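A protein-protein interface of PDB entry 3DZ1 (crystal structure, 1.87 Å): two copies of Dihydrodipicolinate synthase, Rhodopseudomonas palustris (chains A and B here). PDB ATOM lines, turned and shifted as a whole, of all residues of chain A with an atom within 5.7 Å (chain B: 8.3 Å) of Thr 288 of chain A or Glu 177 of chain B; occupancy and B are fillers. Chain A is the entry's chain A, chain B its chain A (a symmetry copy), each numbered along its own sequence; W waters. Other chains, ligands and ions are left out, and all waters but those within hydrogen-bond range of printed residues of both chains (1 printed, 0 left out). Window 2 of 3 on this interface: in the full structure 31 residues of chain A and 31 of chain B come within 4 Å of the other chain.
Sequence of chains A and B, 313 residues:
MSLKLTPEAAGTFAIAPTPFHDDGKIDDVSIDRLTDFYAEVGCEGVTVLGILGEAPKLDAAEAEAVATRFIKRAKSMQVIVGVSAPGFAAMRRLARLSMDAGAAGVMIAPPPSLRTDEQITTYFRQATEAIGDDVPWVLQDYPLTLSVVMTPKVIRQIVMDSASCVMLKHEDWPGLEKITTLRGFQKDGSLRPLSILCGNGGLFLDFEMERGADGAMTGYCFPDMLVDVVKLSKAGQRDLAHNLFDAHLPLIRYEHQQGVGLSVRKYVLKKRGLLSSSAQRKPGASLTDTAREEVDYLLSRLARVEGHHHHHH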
ATOM      1  N   SER A 286     -20.301  28.830   3.226  1.00  0.00           N
ATOM      2  CA  SER A 286     -19.445  29.339   2.160  1.00  0.00           C
ATOM      3  C   SER A 286     -18.005  29.517   2.645  1.00  0.00           C
ATOM      4  O   SER A 286     -17.722  29.422   3.840  1.00  0.00           O
ATOM      5  CB  SER A 286     -19.987  30.675   1.649  1.00  0.00           C
ATOM      6  OG  SER A 286     -19.180  31.176   0.599  1.00  0.00           O
ATOM      7  N   LEU A 287     -17.097  29.772   1.711  1.00  0.00           N
ATOM      8  CA  LEU A 287     -15.693  29.958   2.053  1.00  0.00           C
ATOM      9  C   LEU A 287     -15.453  31.271   2.789  1.00  0.00           C
ATOM     10  O   LEU A 287     -16.088  32.285   2.491  1.00  0.00           O
ATOM     11  CB  LEU A 287     -14.830  29.948   0.788  1.00  0.00           C
ATOM     12  CG  LEU A 287     -14.793  28.683  -0.068  1.00  0.00           C
ATOM     13  CD1 LEU A 287     -13.997  28.963  -1.334  1.00  0.00           C
ATOM     14  CD2 LEU A 287     -14.177  27.536   0.719  1.00  0.00           C
ATOM     15  N   THR A 288     -14.535  31.245   3.751  1.00  0.00           N
ATOM     16  CA  THR A 288     -14.177  32.445   4.493  1.00  0.00           C
ATOM     17  C   THR A 288     -13.379  33.308   3.521  1.00  0.00           C
ATOM     18  O   THR A 288     -12.950  32.826   2.469  1.00  0.00           O
ATOM     19  CB  THR A 288     -13.264  32.125   5.689  1.00  0.00           C
ATOM     20  OG1 THR A 288     -12.082  31.466   5.217  1.00  0.00           O
ATOM     21  CG2 THR A 288     -13.972  31.226   6.689  1.00  0.00           C
ATOM     22  N   ASP A 289     -13.180  34.575   3.863  1.00  0.00           N
ATOM     23  CA  ASP A 289     -12.409  35.480   3.012  1.00  0.00           C
ATOM     24  C   ASP A 289     -11.013  34.902   2.765  1.00  0.00           C
ATOM     25  O   ASP A 289     -10.494  34.946   1.651  1.00  0.00           O
ATOM     26  CB  ASP A 289     -12.278  36.853   3.685  1.00  0.00           C
ATOM     27  CG  ASP A 289     -11.662  37.898   2.769  1.00  0.00           C
ATOM     28  OD1 ASP A 289     -12.389  38.444   1.913  1.00  0.00           O
ATOM     29  OD2 ASP A 289     -10.449  38.171   2.900  1.00  0.00           O
ATOM     30  N   THR A 290     -10.411  34.350   3.813  1.00  0.00           N
ATOM     31  CA  THR A 290      -9.074  33.771   3.705  1.00  0.00           C
ATOM     32  C   THR A 290      -9.039  32.544   2.797  1.00  0.00           C
ATOM     33  O   THR A 290      -8.151  32.419   1.959  1.00  0.00           O
ATOM     34  CB  THR A 290      -8.533  33.405   5.095  1.00  0.00           C
ATOM     35  OG1 THR A 290      -8.377  34.607   5.861  1.00  0.00           O
ATOM     36  CG2 THR A 290      -7.190  32.711   4.990  1.00  0.00           C
ATOM     37  N   ALA A 291      -9.999  31.641   2.965  1.00  0.00           N
ATOM     38  CA  ALA A 291     -10.055  30.444   2.132  1.00  0.00           C
ATOM     39  C   ALA A 291     -10.201  30.852   0.665  1.00  0.00           C
ATOM     40  O   ALA A 291      -9.589  30.251  -0.219  1.00  0.00           O
ATOM     41  CB  ALA A 291     -11.222  29.556   2.559  1.00  0.00           C
ATOM     42  N   ARG A 292     -11.005  31.881   0.407  1.00  0.00           N
ATOM     43  CA  ARG A 292     -11.196  32.359  -0.957  1.00  0.00           C
ATOM     44  C   ARG A 292      -9.869  32.843  -1.527  1.00  0.00           C
ATOM     45  O   ARG A 292      -9.548  32.564  -2.679  1.00  0.00           O
ATOM     46  CB  ARG A 292     -12.226  33.499  -1.010  1.00  0.00           C
ATOM     47  CG  ARG A 292     -13.645  33.085  -0.637  1.00  0.00           C
ATOM     48  CD  ARG A 292     -14.669  34.101  -1.136  1.00  0.00           C
ATOM     49  NE  ARG A 292     -14.487  35.434  -0.559  1.00  0.00           N
ATOM     50  CZ  ARG A 292     -14.948  35.805   0.632  1.00  0.00           C
ATOM     51  NH1 ARG A 292     -15.623  34.945   1.381  1.00  0.00           N
ATOM     52  NH2 ARG A 292     -14.747  37.042   1.070  1.00  0.00           N
ATOM     53  N   GLU A 293      -9.096  33.563  -0.718  1.00  0.00           N
ATOM     54  CA  GLU A 293      -7.796  34.068  -1.156  1.00  0.00           C
ATOM     55  C   GLU A 293      -6.865  32.898  -1.470  1.00  0.00           C
ATOM     56  O   GLU A 293      -6.148  32.911  -2.472  1.00  0.00           O
ATOM     57  CB  GLU A 293      -7.166  34.945  -0.064  1.00  0.00           C
ATOM     58  CG  GLU A 293      -5.900  35.697  -0.484  1.00  0.00           C
ATOM     59  CD  GLU A 293      -4.704  34.791  -0.726  1.00  0.00           C
ATOM     60  OE1 GLU A 293      -4.541  33.815   0.029  1.00  0.00           O
ATOM     61  OE2 GLU A 293      -3.913  35.063  -1.657  1.00  0.00           O
ATOM     62  N   GLU A 294      -6.875  31.889  -0.605  1.00  0.00           N
ATOM     63  CA  GLU A 294      -6.025  30.718  -0.804  1.00  0.00           C
ATOM     64  C   GLU A 294      -6.388  30.015  -2.107  1.00  0.00           C
ATOM     65  O   GLU A 294      -5.507  29.595  -2.854  1.00  0.00           O
ATOM     66  CB  GLU A 294      -6.155  29.759   0.384  1.00  0.00           C
ATOM     67  CG  GLU A 294      -5.794  30.413   1.720  1.00  0.00           C
ATOM     68  CD  GLU A 294      -6.001  29.501   2.910  1.00  0.00           C
ATOM     69  OE1 GLU A 294      -7.013  28.774   2.931  1.00  0.00           O
ATOM     70  OE2 GLU A 294      -5.160  29.524   3.833  1.00  0.00           O
ATOM     71  N   PRO B 152     -12.574  23.933  18.328  1.00  0.00           N
ATOM     72  CA  PRO B 152     -11.535  24.812  18.864  1.00  0.00           C
ATOM     73  C   PRO B 152     -11.798  25.137  20.333  1.00  0.00           C
ATOM     74  O   PRO B 152     -10.870  25.197  21.130  1.00  0.00           O
ATOM     75  CB  PRO B 152     -11.634  26.036  17.964  1.00  0.00           C
ATOM     76  CG  PRO B 152     -11.955  25.420  16.639  1.00  0.00           C
ATOM     77  CD  PRO B 152     -13.019  24.396  17.002  1.00  0.00           C
ATOM     78  N   HIS B 170      -1.914  19.241  15.218  1.00  0.00           N
ATOM     79  CA  HIS B 170      -3.050  19.547  14.359  1.00  0.00           C
ATOM     80  C   HIS B 170      -3.163  18.664  13.121  1.00  0.00           C
ATOM     81  O   HIS B 170      -2.360  18.773  12.191  1.00  0.00           O
ATOM     82  CB  HIS B 170      -2.967  21.021  13.949  1.00  0.00           C
ATOM     83  CG  HIS B 170      -4.036  21.454  12.996  1.00  0.00           C
ATOM     84  ND1 HIS B 170      -5.310  21.789  13.402  1.00  0.00           N
ATOM     85  CD2 HIS B 170      -4.019  21.609  11.651  1.00  0.00           C
ATOM     86  CE1 HIS B 170      -6.032  22.129  12.350  1.00  0.00           C
ATOM     87  NE2 HIS B 170      -5.272  22.028  11.275  1.00  0.00           N
ATOM     88  N   ASP B 172      -6.609  17.901  11.909  1.00  0.00           N
ATOM     89  CA  ASP B 172      -8.000  17.985  11.471  1.00  0.00           C
ATOM     90  C   ASP B 172      -8.028  18.224   9.964  1.00  0.00           C
ATOM     91  O   ASP B 172      -7.130  18.865   9.404  1.00  0.00           O
ATOM     92  CB  ASP B 172      -8.744  19.110  12.192  1.00  0.00           C
ATOM     93  CG  ASP B 172     -10.249  18.927  12.141  1.00  0.00           C
ATOM     94  OD1 ASP B 172     -10.704  17.957  11.497  1.00  0.00           O
ATOM     95  OD2 ASP B 172     -10.977  19.743  12.742  1.00  0.00           O
ATOM     96  N   PRO B 174     -11.206  19.000   7.068  1.00  0.00           N
ATOM     97  CA  PRO B 174     -10.540  20.306   6.925  1.00  0.00           C
ATOM     98  C   PRO B 174     -10.174  20.928   8.271  1.00  0.00           C
ATOM     99  O   PRO B 174     -10.969  20.895   9.209  1.00  0.00           O
ATOM    100  CB  PRO B 174     -11.583  21.156   6.186  1.00  0.00           C
ATOM    101  CG  PRO B 174     -12.470  20.133   5.513  1.00  0.00           C
ATOM    102  CD  PRO B 174     -12.587  19.070   6.568  1.00  0.00           C
ATOM    103  N   GLY B 175      -8.986  21.517   8.359  1.00  0.00           N
ATOM    104  CA  GLY B 175      -8.575  22.120   9.613  1.00  0.00           C
ATOM    105  C   GLY B 175      -7.925  23.488   9.522  1.00  0.00           C
ATOM    106  O   GLY B 175      -7.440  24.005  10.524  1.00  0.00           O
ATOM    107  N   LEU B 176      -7.911  24.096   8.340  1.00  0.00           N
ATOM    108  CA  LEU B 176      -7.281  25.407   8.223  1.00  0.00           C
ATOM    109  C   LEU B 176      -7.946  26.460   9.112  1.00  0.00           C
ATOM    110  O   LEU B 176      -7.257  27.229   9.789  1.00  0.00           O
ATOM    111  CB  LEU B 176      -7.274  25.873   6.762  1.00  0.00           C
ATOM    112  CG  LEU B 176      -6.378  25.058   5.818  1.00  0.00           C
ATOM    113  CD1 LEU B 176      -6.440  25.638   4.411  1.00  0.00           C
ATOM    114  CD2 LEU B 176      -4.936  25.068   6.335  1.00  0.00           C
ATOM    115  N   GLU B 177      -9.278  26.493   9.131  1.00  0.00           N
ATOM    116  CA  GLU B 177      -9.978  27.482   9.946  1.00  0.00           C
ATOM    117  C   GLU B 177      -9.754  27.266  11.446  1.00  0.00           C
ATOM    118  O   GLU B 177      -9.779  28.216  12.223  1.00  0.00           O
ATOM    119  CB  GLU B 177     -11.479  27.472   9.642  1.00  0.00           C
ATOM    120  CG  GLU B 177     -11.853  27.832   8.201  1.00  0.00           C
ATOM    121  CD  GLU B 177     -11.292  29.173   7.733  1.00  0.00           C
ATOM    122  OE1 GLU B 177     -11.085  30.079   8.570  1.00  0.00           O
ATOM    123  OE2 GLU B 177     -11.074  29.328   6.510  1.00  0.00           O
ATOM    124  N   LYS B 178      -9.538  26.018  11.851  1.00  0.00           N
ATOM    125  CA  LYS B 178      -9.300  25.715  13.258  1.00  0.00           C
ATOM    126  C   LYS B 178      -8.036  26.420  13.746  1.00  0.00           C
ATOM    127  O   LYS B 178      -7.990  26.931  14.862  1.00  0.00           O
ATOM    128  CB  LYS B 178      -9.178  24.198  13.466  1.00  0.00           C
ATOM    129  CG  LYS B 178      -8.700  23.790  14.854  1.00  0.00           C
ATOM    130  CD  LYS B 178      -8.791  22.280  15.057  1.00  0.00           C
ATOM    131  CE  LYS B 178     -10.226  21.837  15.310  1.00  0.00           C
ATOM    132  NZ  LYS B 178     -10.346  20.355  15.435  1.00  0.00           N
ATOM    133  N   ILE B 179      -7.006  26.450  12.910  1.00  0.00           N
ATOM    134  CA  ILE B 179      -5.769  27.107  13.299  1.00  0.00           C
ATOM    135  C   ILE B 179      -6.050  28.587  13.518  1.00  0.00           C
ATOM    136  O   ILE B 179      -5.688  29.148  14.548  1.00  0.00           O
ATOM    137  CB  ILE B 179      -4.682  26.940  12.221  1.00  0.00           C
ATOM    138  CG1 ILE B 179      -4.370  25.452  12.039  1.00  0.00           C
ATOM    139  CG2 ILE B 179      -3.421  27.705  12.626  1.00  0.00           C
ATOM    140  CD1 ILE B 179      -3.318  25.172  10.985  1.00  0.00           C
ATOM    141  N   THR B 180      -6.710  29.212  12.548  1.00  0.00           N
ATOM    142  CA  THR B 180      -7.047  30.626  12.645  1.00  0.00           C
ATOM    143  C   THR B 180      -7.854  30.921  13.907  1.00  0.00           C
ATOM    144  O   THR B 180      -7.569  31.887  14.616  1.00  0.00           O
ATOM    145  CB  THR B 180      -7.847  31.081  11.408  1.00  0.00           C
ATOM    146  OG1 THR B 180      -7.018  30.951  10.243  1.00  0.00           O
ATOM    147  CG2 THR B 180      -8.300  32.529  11.552  1.00  0.00           C
ATOM    148  N   THR B 181      -8.856  30.089  14.189  1.00  0.00           N
ATOM    149  CA  THR B 181      -9.701  30.278  15.368  1.00  0.00           C
ATOM    150  C   THR B 181      -8.885  30.197  16.661  1.00  0.00           C
ATOM    151  O   THR B 181      -9.027  31.047  17.550  1.00  0.00           O
ATOM    152  CB  THR B 181     -10.834  29.231  15.413  1.00  0.00           C
ATOM    153  OG1 THR B 181     -11.682  29.405  14.274  1.00  0.00           O
ATOM    154  CG2 THR B 181     -11.665  29.385  16.683  1.00  0.00           C
ATOM    155  N   LEU B 182      -8.032  29.182  16.766  1.00  0.00           N
ATOM    156  CA  LEU B 182      -7.187  29.018  17.947  1.00  0.00           C
ATOM    157  C   LEU B 182      -6.238  30.205  18.128  1.00  0.00           C
ATOM    158  O   LEU B 182      -6.044  30.691  19.246  1.00  0.00           O
ATOM    159  CB  LEU B 182      -6.389  27.707  17.864  1.00  0.00           C
ATOM    160  CG  LEU B 182      -7.221  26.421  17.987  1.00  0.00           C
ATOM    161  CD1 LEU B 182      -6.354  25.213  17.717  1.00  0.00           C
ATOM    162  CD2 LEU B 182      -7.843  26.334  19.385  1.00  0.00           C
ATOM    163  N   ARG B 183      -5.642  30.682  17.039  1.00  0.00           N
ATOM    164  CA  ARG B 183      -4.744  31.827  17.152  1.00  0.00           C
ATOM    165  C   ARG B 183      -5.546  33.042  17.615  1.00  0.00           C
ATOM    166  O   ARG B 183      -5.029  33.915  18.322  1.00  0.00           O
ATOM    167  CB  ARG B 183      -4.063  32.116  15.812  1.00  0.00           C
ATOM    168  CG  ARG B 183      -3.027  31.065  15.411  1.00  0.00           C
ATOM    169  CD  ARG B 183      -1.986  30.848  16.516  1.00  0.00           C
ATOM    170  NE  ARG B 183      -0.919  29.935  16.104  1.00  0.00           N
ATOM    171  CZ  ARG B 183      -0.152  29.245  16.945  1.00  0.00           C
ATOM    172  NH1 ARG B 183      -0.329  29.356  18.253  1.00  0.00           N
ATOM    173  NH2 ARG B 183       0.789  28.433  16.478  1.00  0.00           N
ATOM    174  N   GLY B 184      -6.813  33.080  17.223  1.00  0.00           N
ATOM    175  CA  GLY B 184      -7.686  34.173  17.616  1.00  0.00           C
ATOM    176  C   GLY B 184      -7.956  34.158  19.111  1.00  0.00           C
ATOM    177  O   GLY B 184      -8.045  35.216  19.744  1.00  0.00           O
ATOM    178  N   PHE B 207      -0.536  25.778   3.408  1.00  0.00           N
ATOM    179  CA  PHE B 207      -1.451  26.782   3.929  1.00  0.00           C
ATOM    180  C   PHE B 207      -1.506  26.798   5.452  1.00  0.00           C
ATOM    181  O   PHE B 207      -1.811  27.824   6.052  1.00  0.00           O
ATOM    182  CB  PHE B 207      -2.846  26.575   3.331  1.00  0.00           C
ATOM    183  CG  PHE B 207      -2.942  26.981   1.883  1.00  0.00           C
ATOM    184  CD1 PHE B 207      -2.776  28.314   1.510  1.00  0.00           C
ATOM    185  CD2 PHE B 207      -3.169  26.034   0.889  1.00  0.00           C
ATOM    186  CE1 PHE B 207      -2.832  28.695   0.171  1.00  0.00           C
ATOM    187  CE2 PHE B 207      -3.227  26.405  -0.454  1.00  0.00           C
ATOM    188  CZ  PHE B 207      -3.058  27.740  -0.813  1.00  0.00           C
ATOM    189  N   GLU B 208      -1.201  25.668   6.080  1.00  0.00           N
ATOM    190  CA  GLU B 208      -1.216  25.612   7.533  1.00  0.00           C
ATOM    191  C   GLU B 208      -0.179  26.577   8.101  1.00  0.00           C
ATOM    192  O   GLU B 208      -0.410  27.210   9.129  1.00  0.00           O
ATOM    193  CB  GLU B 208      -0.949  24.183   8.012  1.00  0.00           C
ATOM    194  CG  GLU B 208      -2.168  23.281   7.883  1.00  0.00           C
ATOM    195  CD  GLU B 208      -1.823  21.812   7.954  1.00  0.00           C
ATOM    196  OE1 GLU B 208      -2.744  21.003   8.199  1.00  0.00           O
ATOM    197  OE2 GLU B 208      -0.638  21.469   7.758  1.00  0.00           O
ATOM    198  N   ARG B 211      -1.581  30.030   7.958  1.00  0.00           N
ATOM    199  CA  ARG B 211      -2.599  30.262   8.978  1.00  0.00           C
ATOM    200  C   ARG B 211      -1.990  30.573  10.340  1.00  0.00           C
ATOM    201  O   ARG B 211      -2.657  31.138  11.209  1.00  0.00           O
ATOM    202  CB  ARG B 211      -3.514  29.047   9.113  1.00  0.00           C
ATOM    203  CG  ARG B 211      -4.364  28.774   7.887  1.00  0.00           C
ATOM    204  CD  ARG B 211      -5.243  29.961   7.557  1.00  0.00           C
ATOM    205  NE  ARG B 211      -6.146  29.664   6.448  1.00  0.00           N
ATOM    206  CZ  ARG B 211      -7.471  29.703   6.538  1.00  0.00           C
ATOM    207  NH1 ARG B 211      -8.050  30.029   7.686  1.00  0.00           N
ATOM    208  NH2 ARG B 211      -8.214  29.420   5.478  1.00  0.00           N
HETATM  209  O   HOH W   1     -13.830  28.675   4.651  1.00  0.00           O
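Water W1 bridges the backbone NH of Thr 288 of chain A (2.8 Å) and the side-chain carboxylate of Glu 177 of chain B (3.4 Å).
The side-chain hydroxyl of Thr 288 of chain A sits at hydrogen-bond distance from the side-chain carboxylate of Glu 177 of chain B (2.7 Å).
The side-chain carboxylate (OE2) of Glu 294 of chain A is in salt-bridge range of the guanidinium group (NE) of Arg 211 of chain B, 2.8 Å away.
Among the printed residues, merely in contact across the chains: Thr 290 of chain A with Arg 211 of chain B (3.4 Å), Ala 291 of chain A with Glu 177 of chain B (3.96 Å), Ala 291 of chain A with Arg 211 of chain B (3.8 Å), Glu 294 of chain A with Leu 176 of chain B (3.5 Å) and Glu 294 of chain A with Phe 207 of chain B (3.5 Å).
Of chain B, only Glu 177 (2.7 Å) comes within 4 Å of Thr 288 of chain A.
Of chain A, only Thr 288 and Ala 291 come within 4 Å of Glu 177 of chain B.
Of the printed residues of chain B, Thr 290 of chain A touches Arg 211 (3.4 Å).
Of the printed residues of chain B, Ala 291 of chain A touches Glu 177 and Arg 211.
Gly 184 of chain B touches none of the printed residues of chain A.
Leu 287 of chain A touches none of the printed residues of chain B.
No position is printed for both chains.
Of the 7 pairs that touch across the chains among the printed residues, none has its exchanged pair printed and touching as well.
OG1 of Thr 288 of chain A is in hydrogen-bond range of N of Ala 291 of chain A (3.1 Å).
The backbone carbonyl oxygen of Glu 177 of chain B lies within hydrogen-bond range of the side-chain hydroxyl of Thr 181 of chain B, 3.0 Å away.
OE2 of Glu 177 of chain B is in salt-bridge range of NH2 of Arg 211 of chain B (3.0 Å).
The guanidinium group (NH1) of Arg 211 of chain B is in hydrogen-bond range of the side-chain hydroxyl (OG1) of Thr 180 of chain B (2.9 Å).
Hydrophobic or aromatic side chains of chain A within 4 Å of the printed part of chain B: Ala 291.
Of the 17 printed residues of chain B, 4 touch a printed residue of chain A.
Hydrophobic or aromatic side chains of chain B that line the printed part of chain A: Leu 176 and Phe 207.
Among the printed residues, Asp or Glu carboxylates within 4 Å of a Lys or Arg side-chain nitrogen of the other chain: Glu 294 of chain A with Arg 211 of chain B (2.8 Å).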
